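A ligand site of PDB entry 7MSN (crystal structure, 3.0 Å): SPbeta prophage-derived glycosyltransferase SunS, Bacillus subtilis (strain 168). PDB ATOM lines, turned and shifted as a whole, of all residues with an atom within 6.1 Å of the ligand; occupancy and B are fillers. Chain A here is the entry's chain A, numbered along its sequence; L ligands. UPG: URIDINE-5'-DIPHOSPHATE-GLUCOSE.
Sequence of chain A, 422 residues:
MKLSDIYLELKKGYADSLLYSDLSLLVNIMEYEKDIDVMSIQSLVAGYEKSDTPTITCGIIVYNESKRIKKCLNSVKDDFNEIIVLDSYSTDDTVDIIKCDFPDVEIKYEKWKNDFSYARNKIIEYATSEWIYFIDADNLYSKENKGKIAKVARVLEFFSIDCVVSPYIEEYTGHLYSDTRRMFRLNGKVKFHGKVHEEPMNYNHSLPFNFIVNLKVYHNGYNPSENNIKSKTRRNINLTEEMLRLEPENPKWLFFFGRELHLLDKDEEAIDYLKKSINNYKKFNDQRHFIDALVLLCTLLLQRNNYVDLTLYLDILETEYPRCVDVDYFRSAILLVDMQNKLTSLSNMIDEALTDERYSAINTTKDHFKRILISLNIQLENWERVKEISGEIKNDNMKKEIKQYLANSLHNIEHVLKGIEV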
ATOM      1  N   ILE A  60     -17.683  15.305  -9.584  1.00  0.00           N
ATOM      2  CA  ILE A  60     -17.802  15.352  -8.126  1.00  0.00           C
ATOM      3  C   ILE A  60     -19.095  16.066  -7.796  1.00  0.00           C
ATOM      4  O   ILE A  60     -19.279  17.208  -8.229  1.00  0.00           O
ATOM      5  CB  ILE A  60     -16.659  16.127  -7.457  1.00  0.00           C
ATOM      6  CG1 ILE A  60     -15.280  15.638  -7.890  1.00  0.00           C
ATOM      7  CG2 ILE A  60     -16.787  16.020  -5.967  1.00  0.00           C
ATOM      8  CD1 ILE A  60     -14.150  16.374  -7.175  1.00  0.00           C
ATOM      9  N   ILE A  61     -19.969  15.449  -7.023  1.00  0.00           N
ATOM     10  CA  ILE A  61     -21.085  16.190  -6.433  1.00  0.00           C
ATOM     11  C   ILE A  61     -20.725  16.455  -4.988  1.00  0.00           C
ATOM     12  O   ILE A  61     -19.957  15.696  -4.386  1.00  0.00           O
ATOM     13  CB  ILE A  61     -22.427  15.447  -6.592  1.00  0.00           C
ATOM     14  CG1 ILE A  61     -22.425  14.069  -5.943  1.00  0.00           C
ATOM     15  CG2 ILE A  61     -22.788  15.281  -8.050  1.00  0.00           C
ATOM     16  CD1 ILE A  61     -23.814  13.520  -5.778  1.00  0.00           C
ATOM     17  N   VAL A  62     -21.205  17.580  -4.423  1.00  0.00           N
ATOM     18  CA  VAL A  62     -20.795  17.985  -3.080  1.00  0.00           C
ATOM     19  C   VAL A  62     -21.955  18.647  -2.342  1.00  0.00           C
ATOM     20  O   VAL A  62     -22.858  19.243  -2.942  1.00  0.00           O
ATOM     21  CB  VAL A  62     -19.574  18.951  -3.020  1.00  0.00           C
ATOM     22  CG1 VAL A  62     -18.299  18.334  -3.586  1.00  0.00           C
ATOM     23  CG2 VAL A  62     -19.887  20.293  -3.645  1.00  0.00           C
ATOM     24  N   TYR A  63     -21.923  18.508  -1.015  1.00  0.00           N
ATOM     25  CA  TYR A  63     -22.612  19.359  -0.062  1.00  0.00           C
ATOM     26  C   TYR A  63     -21.539  19.881   0.892  1.00  0.00           C
ATOM     27  O   TYR A  63     -20.366  19.927   0.516  1.00  0.00           O
ATOM     28  CB  TYR A  63     -23.714  18.609   0.674  1.00  0.00           C
ATOM     29  CG  TYR A  63     -24.699  19.512   1.343  1.00  0.00           C
ATOM     30  CD1 TYR A  63     -25.596  20.275   0.609  1.00  0.00           C
ATOM     31  CD2 TYR A  63     -24.752  19.588   2.720  1.00  0.00           C
ATOM     32  CE1 TYR A  63     -26.495  21.106   1.248  1.00  0.00           C
ATOM     33  CE2 TYR A  63     -25.643  20.410   3.354  1.00  0.00           C
ATOM     34  CZ  TYR A  63     -26.511  21.163   2.629  1.00  0.00           C
ATOM     35  OH  TYR A  63     -27.395  21.965   3.299  1.00  0.00           O
ATOM     36  N   ASN A  64     -21.918  20.283   2.111  1.00  0.00           N
ATOM     37  CA  ASN A  64     -20.960  20.805   3.077  1.00  0.00           C
ATOM     38  C   ASN A  64     -19.711  19.938   3.196  1.00  0.00           C
ATOM     39  O   ASN A  64     -19.641  19.058   4.046  1.00  0.00           O
ATOM     40  CB  ASN A  64     -21.602  20.950   4.458  1.00  0.00           C
ATOM     41  CG  ASN A  64     -22.785  21.889   4.466  1.00  0.00           C
ATOM     42  OD1 ASN A  64     -23.255  22.335   3.414  1.00  0.00           O
ATOM     43  ND2 ASN A  64     -23.284  22.205   5.665  1.00  0.00           N
ATOM     44  N   GLU A  65     -18.724  20.188   2.339  1.00  0.00           N
ATOM     45  CA  GLU A  65     -17.516  19.366   2.345  1.00  0.00           C
ATOM     46  C   GLU A  65     -16.278  20.205   2.577  1.00  0.00           C
ATOM     47  O   GLU A  65     -15.308  20.097   1.815  1.00  0.00           O
ATOM     48  CB  GLU A  65     -17.370  18.596   1.031  1.00  0.00           C
ATOM     49  CG  GLU A  65     -18.448  17.537   0.831  1.00  0.00           C
ATOM     50  CD  GLU A  65     -18.268  16.284   1.669  1.00  0.00           C
ATOM     51  OE1 GLU A  65     -17.298  16.210   2.455  1.00  0.00           O
ATOM     52  OE2 GLU A  65     -19.136  15.384   1.547  1.00  0.00           O
ATOM     53  N   LEU A  86     -20.195  19.741  -8.949  1.00  0.00           N
ATOM     54  CA  LEU A  86     -21.577  20.205  -8.817  1.00  0.00           C
ATOM     55  C   LEU A  86     -21.923  20.399  -7.342  1.00  0.00           C
ATOM     56  O   LEU A  86     -22.152  19.426  -6.619  1.00  0.00           O
ATOM     57  CB  LEU A  86     -22.540  19.231  -9.490  1.00  0.00           C
ATOM     58  CG  LEU A  86     -24.030  19.608  -9.480  1.00  0.00           C
ATOM     59  CD1 LEU A  86     -24.663  19.322 -10.824  1.00  0.00           C
ATOM     60  CD2 LEU A  86     -24.790  18.884  -8.363  1.00  0.00           C
ATOM     61  N   SER A  88     -24.508  21.794  -4.356  1.00  0.00           N
ATOM     62  CA  SER A  88     -25.946  21.695  -4.138  1.00  0.00           C
ATOM     63  C   SER A  88     -26.469  22.791  -3.233  1.00  0.00           C
ATOM     64  O   SER A  88     -27.497  22.627  -2.560  1.00  0.00           O
ATOM     65  CB  SER A  88     -26.282  20.321  -3.560  1.00  0.00           C
ATOM     66  OG  SER A  88     -25.639  19.324  -4.325  1.00  0.00           O
ATOM     67  N   TRP A 112     -30.552  20.881  -4.971  1.00  0.00           N
ATOM     68  CA  TRP A 112     -30.599  19.471  -4.576  1.00  0.00           C
ATOM     69  C   TRP A 112     -32.027  18.963  -4.557  1.00  0.00           C
ATOM     70  O   TRP A 112     -32.812  19.310  -3.663  1.00  0.00           O
ATOM     71  CB  TRP A 112     -29.950  19.239  -3.214  1.00  0.00           C
ATOM     72  CG  TRP A 112     -29.967  17.760  -2.868  1.00  0.00           C
ATOM     73  CD1 TRP A 112     -30.789  17.127  -1.963  1.00  0.00           C
ATOM     74  CD2 TRP A 112     -29.180  16.729  -3.469  1.00  0.00           C
ATOM     75  NE1 TRP A 112     -30.537  15.778  -1.961  1.00  0.00           N
ATOM     76  CE2 TRP A 112     -29.558  15.508  -2.882  1.00  0.00           C
ATOM     77  CE3 TRP A 112     -28.192  16.715  -4.461  1.00  0.00           C
ATOM     78  CZ2 TRP A 112     -28.975  14.308  -3.239  1.00  0.00           C
ATOM     79  CZ3 TRP A 112     -27.618  15.531  -4.805  1.00  0.00           C
ATOM     80  CH2 TRP A 112     -28.007  14.342  -4.202  1.00  0.00           C
ATOM     81  N   ASN A 114     -33.821  15.356  -3.924  1.00  0.00           N
ATOM     82  CA  ASN A 114     -33.391  14.081  -3.351  1.00  0.00           C
ATOM     83  C   ASN A 114     -33.286  12.962  -4.390  1.00  0.00           C
ATOM     84  O   ASN A 114     -34.159  12.085  -4.445  1.00  0.00           O
ATOM     85  CB  ASN A 114     -34.307  13.660  -2.209  1.00  0.00           C
ATOM     86  CG  ASN A 114     -34.152  14.553  -1.008  1.00  0.00           C
ATOM     87  OD1 ASN A 114     -35.079  15.279  -0.636  1.00  0.00           O
ATOM     88  ND2 ASN A 114     -32.989  14.466  -0.370  1.00  0.00           N
ATOM     89  N   PHE A 116     -29.751  11.127  -6.128  1.00  0.00           N
ATOM     90  CA  PHE A 116     -28.325  11.079  -6.423  1.00  0.00           C
ATOM     91  C   PHE A 116     -28.058  10.802  -7.891  1.00  0.00           C
ATOM     92  O   PHE A 116     -27.079  11.302  -8.442  1.00  0.00           O
ATOM     93  CB  PHE A 116     -27.657  10.008  -5.561  1.00  0.00           C
ATOM     94  CG  PHE A 116     -27.318  10.481  -4.195  1.00  0.00           C
ATOM     95  CD1 PHE A 116     -26.059  10.970  -3.928  1.00  0.00           C
ATOM     96  CD2 PHE A 116     -28.253  10.440  -3.177  1.00  0.00           C
ATOM     97  CE1 PHE A 116     -25.732  11.403  -2.668  1.00  0.00           C
ATOM     98  CE2 PHE A 116     -27.934  10.871  -1.906  1.00  0.00           C
ATOM     99  CZ  PHE A 116     -26.660  11.368  -1.653  1.00  0.00           C
ATOM    100  N   ALA A 119     -28.272  14.204  -9.798  1.00  0.00           N
ATOM    101  CA  ALA A 119     -27.084  15.030  -9.692  1.00  0.00           C
ATOM    102  C   ALA A 119     -25.991  14.509 -10.615  1.00  0.00           C
ATOM    103  O   ALA A 119     -25.208  15.294 -11.169  1.00  0.00           O
ATOM    104  CB  ALA A 119     -26.584  15.081  -8.245  1.00  0.00           C
ATOM    105  N   ARG A 120     -25.960  13.202 -10.824  1.00  0.00           N
ATOM    106  CA  ARG A 120     -24.968  12.562 -11.674  1.00  0.00           C
ATOM    107  C   ARG A 120     -25.265  12.821 -13.146  1.00  0.00           C
ATOM    108  O   ARG A 120     -24.336  12.962 -13.944  1.00  0.00           O
ATOM    109  CB  ARG A 120     -24.918  11.067 -11.347  1.00  0.00           C
ATOM    110  CG  ARG A 120     -24.520  10.812  -9.902  1.00  0.00           C
ATOM    111  CD  ARG A 120     -23.070  11.096  -9.691  1.00  0.00           C
ATOM    112  NE  ARG A 120     -22.680  11.042  -8.286  1.00  0.00           N
ATOM    113  CZ  ARG A 120     -22.314   9.976  -7.634  1.00  0.00           C
ATOM    114  NH1 ARG A 120     -22.354   8.808  -8.248  1.00  0.00           N
ATOM    115  NH2 ARG A 120     -21.959  10.080  -6.373  1.00  0.00           N
ATOM    116  N   ILE A 135     -15.990  10.510  -8.424  1.00  0.00           N
ATOM    117  CA  ILE A 135     -15.289  10.388  -7.158  1.00  0.00           C
ATOM    118  C   ILE A 135     -16.063  11.186  -6.122  1.00  0.00           C
ATOM    119  O   ILE A 135     -16.874  12.049  -6.452  1.00  0.00           O
ATOM    120  CB  ILE A 135     -13.820  10.869  -7.238  1.00  0.00           C
ATOM    121  CG1 ILE A 135     -12.998  10.191  -6.152  1.00  0.00           C
ATOM    122  CG2 ILE A 135     -13.756  12.359  -7.106  1.00  0.00           C
ATOM    123  CD1 ILE A 135     -11.522  10.374  -6.276  1.00  0.00           C
ATOM    124  N   ASP A 136     -15.855  10.852  -4.860  1.00  0.00           N
ATOM    125  CA  ASP A 136     -16.620  11.438  -3.779  1.00  0.00           C
ATOM    126  C   ASP A 136     -15.688  12.236  -2.887  1.00  0.00           C
ATOM    127  O   ASP A 136     -14.462  12.021  -2.892  1.00  0.00           O
ATOM    128  CB  ASP A 136     -17.366  10.338  -2.997  1.00  0.00           C
ATOM    129  CG  ASP A 136     -18.479   9.698  -3.814  1.00  0.00           C
ATOM    130  OD1 ASP A 136     -19.351  10.451  -4.307  1.00  0.00           O
ATOM    131  OD2 ASP A 136     -18.469   8.449  -3.978  1.00  0.00           O
ATOM    132  N   ALA A 137     -16.255  13.182  -2.131  1.00  0.00           N
ATOM    133  CA  ALA A 137     -15.413  14.091  -1.350  1.00  0.00           C
ATOM    134  C   ALA A 137     -14.548  13.357  -0.319  1.00  0.00           C
ATOM    135  O   ALA A 137     -13.419  13.780  -0.026  1.00  0.00           O
ATOM    136  CB  ALA A 137     -16.284  15.150  -0.680  1.00  0.00           C
ATOM    137  N   ASP A 138     -15.034  12.244   0.239  1.00  0.00           N
ATOM    138  CA  ASP A 138     -14.281  11.507   1.248  1.00  0.00           C
ATOM    139  C   ASP A 138     -13.363  10.441   0.658  1.00  0.00           C
ATOM    140  O   ASP A 138     -12.924   9.550   1.388  1.00  0.00           O
ATOM    141  CB  ASP A 138     -15.249  10.926   2.294  1.00  0.00           C
ATOM    142  CG  ASP A 138     -16.326  10.000   1.698  1.00  0.00           C
ATOM    143  OD1 ASP A 138     -16.290   8.775   1.967  1.00  0.00           O
ATOM    144  OD2 ASP A 138     -17.261  10.510   1.041  1.00  0.00           O
ATOM    145  N   ASN A 139     -12.984  10.555  -0.612  1.00  0.00           N
ATOM    146  CA  ASN A 139     -12.035   9.632  -1.215  1.00  0.00           C
ATOM    147  C   ASN A 139     -10.781  10.367  -1.704  1.00  0.00           C
ATOM    148  O   ASN A 139     -10.789  11.575  -1.949  1.00  0.00           O
ATOM    149  CB  ASN A 139     -12.694   8.884  -2.390  1.00  0.00           C
ATOM    150  CG  ASN A 139     -13.730   7.857  -1.927  1.00  0.00           C
ATOM    151  OD1 ASN A 139     -13.697   7.399  -0.784  1.00  0.00           O
ATOM    152  ND2 ASN A 139     -14.657   7.506  -2.817  1.00  0.00           N
ATOM    153  N   ARG A 182     -17.663   3.410 -11.760  1.00  0.00           N
ATOM    154  CA  ARG A 182     -17.366   4.826 -11.607  1.00  0.00           C
ATOM    155  C   ARG A 182     -16.992   5.505 -12.900  1.00  0.00           C
ATOM    156  O   ARG A 182     -17.031   6.739 -12.976  1.00  0.00           O
ATOM    157  CB  ARG A 182     -16.219   5.038 -10.611  1.00  0.00           C
ATOM    158  CG  ARG A 182     -16.531   4.845  -9.123  1.00  0.00           C
ATOM    159  CD  ARG A 182     -17.909   5.329  -8.699  1.00  0.00           C
ATOM    160  NE  ARG A 182     -17.841   5.811  -7.319  1.00  0.00           N
ATOM    161  CZ  ARG A 182     -18.198   5.119  -6.227  1.00  0.00           C
ATOM    162  NH1 ARG A 182     -18.632   3.867  -6.329  1.00  0.00           N
ATOM    163  NH2 ARG A 182     -18.099   5.676  -5.029  1.00  0.00           N
ATOM    164  N   LYS A 195     -32.961   6.887  -6.944  1.00  0.00           N
ATOM    165  CA  LYS A 195     -32.813   8.053  -6.082  1.00  0.00           C
ATOM    166  C   LYS A 195     -31.589   7.930  -5.183  1.00  0.00           C
ATOM    167  O   LYS A 195     -30.819   8.883  -5.032  1.00  0.00           O
ATOM    168  CB  LYS A 195     -34.090   8.291  -5.254  1.00  0.00           C
ATOM    169  CG  LYS A 195     -35.232   9.026  -5.998  1.00  0.00           C
ATOM    170  CD  LYS A 195     -36.664   8.739  -5.421  1.00  0.00           C
ATOM    171  CE  LYS A 195     -37.077   9.608  -4.205  1.00  0.00           C
ATOM    172  NZ  LYS A 195     -37.223  11.071  -4.522  1.00  0.00           N
ATOM    173  N   VAL A 196     -31.372   6.734  -4.609  1.00  0.00           N
ATOM    174  CA  VAL A 196     -30.217   6.451  -3.749  1.00  0.00           C
ATOM    175  C   VAL A 196     -29.674   5.087  -4.153  1.00  0.00           C
ATOM    176  O   VAL A 196     -30.377   4.284  -4.772  1.00  0.00           O
ATOM    177  CB  VAL A 196     -30.611   6.447  -2.254  1.00  0.00           C
ATOM    178  CG1 VAL A 196     -31.601   5.332  -1.967  1.00  0.00           C
ATOM    179  CG2 VAL A 196     -29.380   6.399  -1.340  1.00  0.00           C
ATOM    180  N   HIS A 197     -28.419   4.819  -3.783  1.00  0.00           N
ATOM    181  CA  HIS A 197     -27.703   3.613  -4.217  1.00  0.00           C
ATOM    182  C   HIS A 197     -27.707   3.541  -5.730  1.00  0.00           C
ATOM    183  O   HIS A 197     -27.957   2.499  -6.337  1.00  0.00           O
ATOM    184  CB  HIS A 197     -28.276   2.326  -3.609  1.00  0.00           C
ATOM    185  CG  HIS A 197     -28.114   2.240  -2.126  1.00  0.00           C
ATOM    186  ND1 HIS A 197     -26.908   1.922  -1.532  1.00  0.00           N
ATOM    187  CD2 HIS A 197     -28.991   2.425  -1.108  1.00  0.00           C
ATOM    188  CE1 HIS A 197     -27.052   1.925  -0.215  1.00  0.00           C
ATOM    189  NE2 HIS A 197     -28.307   2.228   0.062  1.00  0.00           N
ATOM    190  N   GLU A 198     -27.464   4.694  -6.337  1.00  0.00           N
ATOM    191  CA  GLU A 198     -27.461   4.815  -7.779  1.00  0.00           C
ATOM    192  C   GLU A 198     -26.344   3.988  -8.363  1.00  0.00           C
ATOM    193  O   GLU A 198     -25.273   3.838  -7.767  1.00  0.00           O
ATOM    194  CB  GLU A 198     -27.290   6.278  -8.181  1.00  0.00           C
ATOM    195  CG  GLU A 198     -25.913   6.862  -7.877  1.00  0.00           C
ATOM    196  CD  GLU A 198     -25.713   7.252  -6.417  1.00  0.00           C
ATOM    197  OE1 GLU A 198     -26.617   7.029  -5.579  1.00  0.00           O
ATOM    198  OE2 GLU A 198     -24.613   7.753  -6.114  1.00  0.00           O
ATOM    199  N   ASN A 228     -20.142  11.336  11.299  1.00  0.00           N
ATOM    200  CA  ASN A 228     -20.972  11.722  10.153  1.00  0.00           C
ATOM    201  C   ASN A 228     -21.751  10.530   9.595  1.00  0.00           C
ATOM    202  O   ASN A 228     -22.796  10.730   8.971  1.00  0.00           O
ATOM    203  CB  ASN A 228     -20.086  12.361   9.088  1.00  0.00           C
ATOM    204  CG  ASN A 228     -19.055  11.382   8.480  1.00  0.00           C
ATOM    205  OD1 ASN A 228     -18.449  10.549   9.181  1.00  0.00           O
ATOM    206  ND2 ASN A 228     -18.803  11.516   7.173  1.00  0.00           N
ATOM    207  N   LYS A 232     -25.303  10.639   7.672  1.00  0.00           N
ATOM    208  CA  LYS A 232     -25.408  10.177   6.289  1.00  0.00           C
ATOM    209  C   LYS A 232     -26.444   9.075   6.177  1.00  0.00           C
ATOM    210  O   LYS A 232     -27.319   9.094   5.293  1.00  0.00           O
ATOM    211  CB  LYS A 232     -24.054   9.685   5.773  1.00  0.00           C
ATOM    212  CG  LYS A 232     -22.997  10.726   5.712  1.00  0.00           C
ATOM    213  CD  LYS A 232     -21.903  10.396   4.722  1.00  0.00           C
ATOM    214  CE  LYS A 232     -20.680   9.774   5.371  1.00  0.00           C
ATOM    215  NZ  LYS A 232     -19.537   9.679   4.409  1.00  0.00           N
ATOM    216  N   THR A 233     -26.377   8.108   7.090  1.00  0.00           N
ATOM    217  CA  THR A 233     -27.301   6.983   7.039  1.00  0.00           C
ATOM    218  C   THR A 233     -28.727   7.435   7.209  1.00  0.00           C
ATOM    219  O   THR A 233     -29.624   6.937   6.538  1.00  0.00           O
ATOM    220  CB  THR A 233     -26.941   5.984   8.118  1.00  0.00           C
ATOM    221  OG1 THR A 233     -25.543   5.726   8.039  1.00  0.00           O
ATOM    222  CG2 THR A 233     -27.715   4.696   7.921  1.00  0.00           C
ATOM    223  N   ARG A 235     -30.119  10.178   6.431  1.00  0.00           N
ATOM    224  CA  ARG A 235     -30.537  10.727   5.147  1.00  0.00           C
ATOM    225  C   ARG A 235     -30.775   9.648   4.096  1.00  0.00           C
ATOM    226  O   ARG A 235     -31.800   9.646   3.409  1.00  0.00           O
ATOM    227  CB  ARG A 235     -29.472  11.685   4.635  1.00  0.00           C
ATOM    228  CG  ARG A 235     -29.662  12.079   3.198  1.00  0.00           C
ATOM    229  CD  ARG A 235     -28.346  12.566   2.607  1.00  0.00           C
ATOM    230  NE  ARG A 235     -27.484  11.478   2.163  1.00  0.00           N
ATOM    231  CZ  ARG A 235     -26.165  11.603   2.000  1.00  0.00           C
ATOM    232  NH1 ARG A 235     -25.581  12.753   2.260  1.00  0.00           N
ATOM    233  NH2 ARG A 235     -25.430  10.571   1.593  1.00  0.00           N
ATOM    234  N   ASN A 236     -29.801   8.755   3.911  1.00  0.00           N
ATOM    235  CA  ASN A 236     -29.925   7.737   2.881  1.00  0.00           C
ATOM    236  C   ASN A 236     -31.108   6.816   3.138  1.00  0.00           C
ATOM    237  O   ASN A 236     -31.713   6.302   2.179  1.00  0.00           O
ATOM    238  CB  ASN A 236     -28.623   6.961   2.776  1.00  0.00           C
ATOM    239  CG  ASN A 236     -27.560   7.730   2.060  1.00  0.00           C
ATOM    240  OD1 ASN A 236     -26.468   7.954   2.575  1.00  0.00           O
ATOM    241  ND2 ASN A 236     -27.854   8.141   0.837  1.00  0.00           N
HETATM  242  N1  UPG L   1     -23.784  15.220  -1.750  1.00  0.00           N
HETATM  243  C2  UPG L   1     -24.527  15.925  -2.622  1.00  0.00           C
HETATM  244  N3  UPG L   1     -25.739  16.376  -2.324  1.00  0.00           N
HETATM  245  C4  UPG L   1     -26.273  16.139  -1.160  1.00  0.00           C
HETATM  246  C5  UPG L   1     -25.545  15.398  -0.210  1.00  0.00           C
HETATM  247  C6  UPG L   1     -24.260  14.945  -0.546  1.00  0.00           C
HETATM  248  O2  UPG L   1     -24.097  16.175  -3.699  1.00  0.00           O
HETATM  249  O4  UPG L   1     -27.558  16.632  -0.895  1.00  0.00           O
HETATM  250  C1C UPG L   1     -22.437  14.774  -2.189  1.00  0.00           C
HETATM  251  C2C UPG L   1     -21.380  14.400  -1.074  1.00  0.00           C
HETATM  252  O2C UPG L   1     -20.608  15.407  -0.780  1.00  0.00           O
HETATM  253  C3C UPG L   1     -20.503  13.272  -1.749  1.00  0.00           C
HETATM  254  C4C UPG L   1     -21.349  12.633  -2.481  1.00  0.00           C
HETATM  255  O4C UPG L   1     -22.560  13.709  -2.886  1.00  0.00           O
HETATM  256  O3C UPG L   1     -19.368  13.827  -2.539  1.00  0.00           O
HETATM  257  C5C UPG L   1     -22.064  11.569  -1.683  1.00  0.00           C
HETATM  258  O5C UPG L   1     -21.142  11.043  -0.724  1.00  0.00           O
HETATM  259  PA  UPG L   1     -21.561  11.024   0.871  1.00  0.00           P
HETATM  260  O1A UPG L   1     -22.239  12.264   1.358  1.00  0.00           O
HETATM  261  O2A UPG L   1     -20.255  10.724   1.580  1.00  0.00           O
HETATM  262  O3A UPG L   1     -22.693   9.869   1.214  1.00  0.00           O
HETATM  263  PB  UPG L   1     -22.291   8.261   1.363  1.00  0.00           P
HETATM  264  O1B UPG L   1     -23.532   7.580   1.927  1.00  0.00           O
HETATM  265  O2B UPG L   1     -21.044   8.123   2.251  1.00  0.00           O
HETATM  266  O3B UPG L   1     -21.848   7.707  -0.155  1.00  0.00           O
HETATM  267  C1' UPG L   1     -22.425   6.569  -0.738  1.00  0.00           C
HETATM  268  C2' UPG L   1     -21.712   6.384  -2.028  1.00  0.00           C
HETATM  269  C3' UPG L   1     -22.047   7.421  -2.976  1.00  0.00           C
HETATM  270  C4' UPG L   1     -23.495   7.602  -3.184  1.00  0.00           C
HETATM  271  C5' UPG L   1     -24.373   7.732  -1.889  1.00  0.00           C
HETATM  272  C6' UPG L   1     -25.735   7.523  -2.135  1.00  0.00           C
HETATM  273  O2' UPG L   1     -20.276   6.520  -1.719  1.00  0.00           O
HETATM  274  O3' UPG L   1     -21.403   7.139  -4.298  1.00  0.00           O
HETATM  275  O4' UPG L   1     -23.594   8.836  -3.898  1.00  0.00           O
HETATM  276  O5' UPG L   1     -23.874   6.721  -0.858  1.00  0.00           O
HETATM  277  O6' UPG L   1     -26.012   6.364  -2.850  1.00  0.00           O
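Ser 88 touches the ligand.
CD1 of Phe 116 touches O4' of the ligand, 3.3 Å away.
Arg 182 touches the ligand.
Val 196 touches the ligand (CG2 to O6', 3.7 Å).
The indole nitrogen of Trp 112 lies close to the side-chain amide nitrogen of Asn 114 (3.2 Å).
The guanidinium group of Arg 120 is in salt-bridge range of the side-chain carboxylate of Glu 198 (3.3 Å).
The side-chain carboxylate (OD2) of Asp 136 lies within salt-bridge range of the guanidinium group (NH2) of Arg 182 (3.0 Å).
ND2 of Asn 228 lies close to NZ of Lys 232, at 3.4 Å.
The guanidinium group (NH2) of Arg 120 lies within salt-bridge range of the side-chain carboxylate (OD1) of Asp 136, at 3.3 Å.
The side-chain amide oxygen (OD1) of Asn 236 sits close to the backbone carbonyl oxygen (O) of Lys 232, 3.1 Å away.
N of Phe 116 sits at hydrogen-bond distance from O of Lys 195, 2.7 Å away.
The guanidinium group (NH2) of Arg 235 lies within hydrogen-bond range of the side-chain amide oxygen (OD1) of Asn 236.
N of Tyr 63 is in hydrogen-bond range of O2C of the ligand, at 3.4 Å.
OD2 of Asp 136 is in hydrogen-bond range of O3' of the ligand (3.2 Å).
N of Ala 137 sits at hydrogen-bond distance from O3C of the ligand, at 3.2 Å.
The backbone NH (N) of Val 62 sits at hydrogen-bond distance from an oxygen (O2) of the ligand.
The backbone carbonyl oxygen (O) of Ile 61 sits at hydrogen-bond distance from an oxygen (O3C) of the ligand (2.7 Å).
NZ of Lys 232 lies within salt-bridge range of O2B of the ligand, 3.1 Å away.
The guanidinium group (NH1) of Arg 235 is in salt-bridge range of an oxygen (O1A) of the ligand, 3.5 Å away.
The guanidinium group (NH2) of Arg 120 is in hydrogen-bond range of an oxygen (O4') of the ligand.
The side-chain amide oxygen (OD1) of Asn 236 sits close to an oxygen (O1B) of the ligand, at 3.0 Å.
N of His 197 sits at hydrogen-bond distance from O6' of the ligand, 3.0 Å away.
OE2 of Glu 65 lies within hydrogen-bond range of O2C of the ligand (2.8 Å).
The side-chain carboxylate of Asp 138 sits close to an oxygen (O2A) of the ligand (3.0 Å).
The side-chain carboxylate of Glu 198 is in hydrogen-bond range of an oxygen (O4') of the ligand (2.7 Å).
The indole nitrogen (NE1) of Trp 112 sits close to an oxygen (O4) of the ligand.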
